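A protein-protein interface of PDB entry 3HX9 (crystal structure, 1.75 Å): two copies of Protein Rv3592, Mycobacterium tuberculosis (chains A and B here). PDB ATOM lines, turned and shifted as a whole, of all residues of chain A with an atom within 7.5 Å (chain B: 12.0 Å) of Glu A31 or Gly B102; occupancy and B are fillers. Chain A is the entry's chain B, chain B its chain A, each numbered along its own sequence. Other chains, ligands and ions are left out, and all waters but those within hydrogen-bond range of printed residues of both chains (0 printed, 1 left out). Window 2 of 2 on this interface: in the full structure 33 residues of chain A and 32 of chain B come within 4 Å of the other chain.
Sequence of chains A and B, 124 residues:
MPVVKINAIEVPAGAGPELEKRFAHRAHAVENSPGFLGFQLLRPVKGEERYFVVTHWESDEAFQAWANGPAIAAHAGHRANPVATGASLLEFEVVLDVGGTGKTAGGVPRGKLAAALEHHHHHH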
ATOM      1  N   ARG A  26      19.893 -11.819  14.489  1.00  0.00           N
ATOM      2  CA  ARG A  26      19.795 -11.305  15.844  1.00  0.00           C
ATOM      3  C   ARG A  26      20.071 -12.411  16.859  1.00  0.00           C
ATOM      4  O   ARG A  26      19.736 -12.306  18.026  1.00  0.00           O
ATOM      5  CB  ARG A  26      18.411 -10.707  16.068  1.00  0.00           C
ATOM      6  CG  ARG A  26      18.249  -9.382  15.322  1.00  0.00           C
ATOM      7  CD  ARG A  26      16.972  -8.672  15.704  1.00  0.00           C
ATOM      8  NE  ARG A  26      16.793  -7.397  14.979  1.00  0.00           N
ATOM      9  CZ  ARG A  26      17.239  -6.195  15.386  1.00  0.00           C
ATOM     10  NH1 ARG A  26      17.917  -6.032  16.534  1.00  0.00           N
ATOM     11  NH2 ARG A  26      17.006  -5.132  14.633  1.00  0.00           N
ATOM     12  N   ALA A  27      20.681 -13.477  16.365  1.00  0.00           N
ATOM     13  CA  ALA A  27      20.800 -14.730  17.154  1.00  0.00           C
ATOM     14  C   ALA A  27      21.527 -14.541  18.453  1.00  0.00           C
ATOM     15  O   ALA A  27      21.314 -15.281  19.424  1.00  0.00           O
ATOM     16  CB  ALA A  27      21.445 -15.844  16.320  1.00  0.00           C
ATOM     17  N   HIS A  28      22.429 -13.560  18.515  1.00  0.00           N
ATOM     18  CA  HIS A  28      23.219 -13.417  19.745  1.00  0.00           C
ATOM     19  C   HIS A  28      22.722 -12.270  20.584  1.00  0.00           C
ATOM     20  O   HIS A  28      23.415 -11.797  21.482  1.00  0.00           O
ATOM     21  CB  HIS A  28      24.766 -13.295  19.374  1.00  0.00           C
ATOM     22  CG  HIS A  28      25.308 -14.498  18.644  1.00  0.00           C
ATOM     23  ND1 HIS A  28      25.372 -14.569  17.259  1.00  0.00           N
ATOM     24  CD2 HIS A  28      25.739 -15.695  19.104  1.00  0.00           C
ATOM     25  CE1 HIS A  28      25.849 -15.753  16.907  1.00  0.00           C
ATOM     26  NE2 HIS A  28      26.057 -16.459  18.005  1.00  0.00           N
ATOM     27  N   ALA A  29      21.496 -11.817  20.308  1.00  0.00           N
ATOM     28  CA  ALA A  29      20.925 -10.682  21.037  1.00  0.00           C
ATOM     29  C   ALA A  29      20.829 -10.856  22.567  1.00  0.00           C
ATOM     30  O   ALA A  29      20.818  -9.857  23.318  1.00  0.00           O
ATOM     31  CB  ALA A  29      19.562 -10.320  20.440  1.00  0.00           C
ATOM     32  N   VAL A  30      20.723 -12.077  23.048  1.00  0.00           N
ATOM     33  CA  VAL A  30      20.449 -12.312  24.456  1.00  0.00           C
ATOM     34  C   VAL A  30      21.714 -12.793  25.165  1.00  0.00           C
ATOM     35  O   VAL A  30      21.707 -13.028  26.384  1.00  0.00           O
ATOM     36  CB  VAL A  30      19.266 -13.335  24.611  1.00  0.00           C
ATOM     37  CG1 VAL A  30      18.800 -13.496  26.088  1.00  0.00           C
ATOM     38  CG2 VAL A  30      18.109 -12.857  23.731  1.00  0.00           C
ATOM     39  N   GLU A  31      22.782 -12.983  24.394  1.00  0.00           N
ATOM     40  CA  GLU A  31      24.050 -13.544  24.936  1.00  0.00           C
ATOM     41  C   GLU A  31      24.512 -12.817  26.189  1.00  0.00           C
ATOM     42  O   GLU A  31      24.441 -11.559  26.287  1.00  0.00           O
ATOM     43  CB  GLU A  31      25.116 -13.428  23.829  1.00  0.00           C
ATOM     44  CG  GLU A  31      25.998 -14.643  23.586  1.00  0.00           C
ATOM     45  CD  GLU A  31      27.309 -14.272  22.898  1.00  0.00           C
ATOM     46  OE1 GLU A  31      27.515 -14.606  21.710  1.00  0.00           O
ATOM     47  OE2 GLU A  31      28.152 -13.623  23.565  1.00  0.00           O
ATOM     48  N   ASN A  32      24.968 -13.610  27.157  1.00  0.00           N
ATOM     49  CA  ASN A  32      25.480 -13.142  28.405  1.00  0.00           C
ATOM     50  C   ASN A  32      24.465 -12.495  29.296  1.00  0.00           C
ATOM     51  O   ASN A  32      24.857 -11.839  30.238  1.00  0.00           O
ATOM     52  CB  ASN A  32      26.609 -12.114  28.129  1.00  0.00           C
ATOM     53  CG  ASN A  32      27.723 -12.700  27.320  1.00  0.00           C
ATOM     54  OD1 ASN A  32      28.319 -12.027  26.488  1.00  0.00           O
ATOM     55  ND2 ASN A  32      28.025 -13.941  27.556  1.00  0.00           N
ATOM     56  N   SER A  33      23.150 -12.606  29.012  1.00  0.00           N
ATOM     57  CA  SER A  33      22.163 -12.096  29.960  1.00  0.00           C
ATOM     58  C   SER A  33      22.230 -13.017  31.184  1.00  0.00           C
ATOM     59  O   SER A  33      22.427 -14.228  30.994  1.00  0.00           O
ATOM     60  CB  SER A  33      20.732 -12.204  29.409  1.00  0.00           C
ATOM     61  OG  SER A  33      20.566 -11.350  28.308  1.00  0.00           O
ATOM     62  N   PRO A  34      22.027 -12.478  32.414  1.00  0.00           N
ATOM     63  CA  PRO A  34      22.257 -13.319  33.578  1.00  0.00           C
ATOM     64  C   PRO A  34      21.251 -14.496  33.672  1.00  0.00           C
ATOM     65  O   PRO A  34      20.050 -14.314  33.551  1.00  0.00           O
ATOM     66  CB  PRO A  34      22.119 -12.363  34.772  1.00  0.00           C
ATOM     67  CG  PRO A  34      22.288 -10.964  34.200  1.00  0.00           C
ATOM     68  CD  PRO A  34      21.674 -11.089  32.787  1.00  0.00           C
ATOM     69  N   PHE A  36      21.004 -16.826  31.574  1.00  0.00           N
ATOM     70  CA  PHE A  36      20.545 -17.297  30.219  1.00  0.00           C
ATOM     71  C   PHE A  36      21.404 -18.427  29.782  1.00  0.00           C
ATOM     72  O   PHE A  36      22.665 -18.298  29.854  1.00  0.00           O
ATOM     73  CB  PHE A  36      20.709 -16.176  29.222  1.00  0.00           C
ATOM     74  CG  PHE A  36      20.264 -16.540  27.826  1.00  0.00           C
ATOM     75  CD1 PHE A  36      18.993 -17.046  27.611  1.00  0.00           C
ATOM     76  CD2 PHE A  36      21.108 -16.384  26.764  1.00  0.00           C
ATOM     77  CE1 PHE A  36      18.580 -17.398  26.288  1.00  0.00           C
ATOM     78  CE2 PHE A  36      20.706 -16.664  25.409  1.00  0.00           C
ATOM     79  CZ  PHE A  36      19.418 -17.219  25.194  1.00  0.00           C
ATOM     80  N   PHE A  39      19.278 -20.651  23.355  1.00  0.00           N
ATOM     81  CA  PHE A  39      17.955 -20.854  22.744  1.00  0.00           C
ATOM     82  C   PHE A  39      18.060 -21.529  21.411  1.00  0.00           C
ATOM     83  O   PHE A  39      19.100 -21.546  20.796  1.00  0.00           O
ATOM     84  CB  PHE A  39      17.165 -19.529  22.674  1.00  0.00           C
ATOM     85  CG  PHE A  39      17.361 -18.706  21.424  1.00  0.00           C
ATOM     86  CD1 PHE A  39      16.388 -18.731  20.387  1.00  0.00           C
ATOM     87  CD2 PHE A  39      18.475 -17.869  21.292  1.00  0.00           C
ATOM     88  CE1 PHE A  39      16.519 -17.949  19.252  1.00  0.00           C
ATOM     89  CE2 PHE A  39      18.603 -17.047  20.155  1.00  0.00           C
ATOM     90  CZ  PHE A  39      17.628 -17.093  19.140  1.00  0.00           C
ATOM     91  N   TRP A  66      14.886 -10.613  32.857  1.00  0.00           N
ATOM     92  CA  TRP A  66      15.179 -10.280  31.482  1.00  0.00           C
ATOM     93  C   TRP A  66      13.940  -9.825  30.723  1.00  0.00           C
ATOM     94  O   TRP A  66      13.949  -8.750  30.093  1.00  0.00           O
ATOM     95  CB  TRP A  66      15.771 -11.499  30.791  1.00  0.00           C
ATOM     96  CG  TRP A  66      15.962 -11.280  29.345  1.00  0.00           C
ATOM     97  CD1 TRP A  66      16.984 -10.553  28.737  1.00  0.00           C
ATOM     98  CD2 TRP A  66      15.195 -11.862  28.293  1.00  0.00           C
ATOM     99  NE1 TRP A  66      16.862 -10.630  27.353  1.00  0.00           N
ATOM    100  CE2 TRP A  66      15.771 -11.408  27.051  1.00  0.00           C
ATOM    101  CE3 TRP A  66      14.071 -12.695  28.266  1.00  0.00           C
ATOM    102  CZ2 TRP A  66      15.276 -11.807  25.804  1.00  0.00           C
ATOM    103  CZ3 TRP A  66      13.547 -13.058  26.998  1.00  0.00           C
ATOM    104  CH2 TRP A  66      14.154 -12.598  25.804  1.00  0.00           C
ATOM    105  N   LEU B  96      18.349 -22.669  14.261  1.00  0.00           N
ATOM    106  CA  LEU B  96      19.514 -22.193  15.000  1.00  0.00           C
ATOM    107  C   LEU B  96      19.536 -22.701  16.446  1.00  0.00           C
ATOM    108  O   LEU B  96      18.499 -23.007  17.034  1.00  0.00           O
ATOM    109  CB  LEU B  96      19.573 -20.681  15.004  1.00  0.00           C
ATOM    110  CG  LEU B  96      18.591 -19.894  15.814  1.00  0.00           C
ATOM    111  CD1 LEU B  96      19.137 -19.712  17.217  1.00  0.00           C
ATOM    112  CD2 LEU B  96      18.397 -18.511  15.171  1.00  0.00           C
ATOM    113  N   ASP B  97      20.730 -22.804  17.011  1.00  0.00           N
ATOM    114  CA  ASP B  97      20.856 -23.297  18.399  1.00  0.00           C
ATOM    115  C   ASP B  97      22.082 -22.548  18.915  1.00  0.00           C
ATOM    116  O   ASP B  97      23.209 -22.873  18.508  1.00  0.00           O
ATOM    117  CB  ASP B  97      21.100 -24.816  18.394  1.00  0.00           C
ATOM    118  CG  ASP B  97      21.276 -25.369  19.781  1.00  0.00           C
ATOM    119  OD1 ASP B  97      21.381 -24.545  20.747  1.00  0.00           O
ATOM    120  OD2 ASP B  97      21.322 -26.641  19.893  1.00  0.00           O
ATOM    121  N   VAL B  98      21.869 -21.540  19.760  1.00  0.00           N
ATOM    122  CA  VAL B  98      22.992 -20.802  20.346  1.00  0.00           C
ATOM    123  C   VAL B  98      23.071 -21.078  21.823  1.00  0.00           C
ATOM    124  O   VAL B  98      22.061 -21.322  22.521  1.00  0.00           O
ATOM    125  CB  VAL B  98      22.959 -19.263  20.115  1.00  0.00           C
ATOM    126  CG1 VAL B  98      23.036 -18.939  18.624  1.00  0.00           C
ATOM    127  CG2 VAL B  98      21.705 -18.668  20.786  1.00  0.00           C
ATOM    128  N   GLY B  99      24.493 -20.927  22.516  1.00  0.00           N
ATOM    129  CA  GLY B  99      24.487 -21.062  24.000  1.00  0.00           C
ATOM    130  C   GLY B  99      24.182 -19.740  24.631  1.00  0.00           C
ATOM    131  O   GLY B  99      23.751 -18.815  23.909  1.00  0.00           O
ATOM    132  N   GLY B 100      24.452 -19.649  25.939  1.00  0.00           N
ATOM    133  CA  GLY B 100      24.022 -18.514  26.740  1.00  0.00           C
ATOM    134  C   GLY B 100      25.150 -17.475  26.793  1.00  0.00           C
ATOM    135  O   GLY B 100      24.904 -16.308  27.098  1.00  0.00           O
ATOM    136  N   THR B 101      26.378 -17.900  26.471  1.00  0.00           N
ATOM    137  CA  THR B 101      27.565 -17.021  26.627  1.00  0.00           C
ATOM    138  C   THR B 101      28.392 -16.754  25.343  1.00  0.00           C
ATOM    139  O   THR B 101      28.203 -17.411  24.310  1.00  0.00           O
ATOM    140  CB  THR B 101      28.485 -17.593  27.662  1.00  0.00           C
ATOM    141  OG1 THR B 101      28.822 -18.926  27.263  1.00  0.00           O
ATOM    142  CG2 THR B 101      27.784 -17.588  29.048  1.00  0.00           C
ATOM    143  N   GLY B 102      29.308 -15.781  25.419  1.00  0.00           N
ATOM    144  CA  GLY B 102      30.282 -15.503  24.338  1.00  0.00           C
ATOM    145  C   GLY B 102      31.052 -14.202  24.532  1.00  0.00           C
ATOM    146  O   GLY B 102      30.932 -13.549  25.575  1.00  0.00           O
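The backbone carbonyl oxygen of Gly B100 is in hydrogen-bond range of the backbone NH of Asn A32, at 2.7 Å. N of Gly B102 lies close to ND2 of Asn A32. N of Gly B102 sits close to OE2 of Glu A31 (3.1 Å). N of Val B98 lies within hydrogen-bond range of O of Phe A39 (3.0 Å).
OE2 of Glu A31 lies close to OD1 of Asn A32 (3.3 Å).
Among the printed residues, merely in contact across the chains: Ala A27 with Val B98 (3.7 Å), His A28 with Val B98 (3.96 Å), Glu A31 with Gly B100 (3.6 Å), Glu A31 with Thr B101 (3.6 Å), Asn A32 with Thr B101 (3.2 Å), Phe A36 with Gly B100 (3.4 Å), Phe A39 with Leu B96 (3.6 Å) and Phe A39 with Asp B97 (3.4 Å).
Glu A31 touches three residues of chain B. Gly B102 touches just these residues of chain A: Glu A31 and Asn A32. Of chain B, only Val B98 (3.96 Å) comes within 4 Å of His A28. No residue of chain B comes within 4 Å of Ala A29. No residue of chain B comes within 4 Å of Val A30. Of chain B, only Gly B100 (2.7 Å), Thr B101 (3.2 Å) and Gly B102 (3.1 Å) come within 4 Å of Asn A32. Of the printed residues of chain A, Thr B101 touches Glu A31 and Asn A32. Printed residues of chain A within 4 Å of Val B98: Ala A27 (3.7 Å), His A28 (3.96 Å) and Phe A39 (3.0 Å). Of the printed residues of chain B, Ala A27 touches Val B98. Printed residues of chain A within 4 Å of Leu B96: Phe A39 (3.6 Å). Arg A26 touches none of the printed residues of chain B. Trp A66 touches none of the printed residues of chain B. The nearest residue of chain A that does not touch Gly B102 is His A28 (6.9 Å). The nearest printed residue of chain A that does not touch Val B98 is Phe A36 (5.1 Å).
Printed residues of chain A that touch a printed residue of chain B: Ala A27, His A28, Glu A31, Asn A32, Phe A36 and Phe A39. Hydrophobic or aromatic side chains of chain A within 4 Å of the printed part of chain B: His A28, Phe A36 and Phe A39.
No position is printed for both chains.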
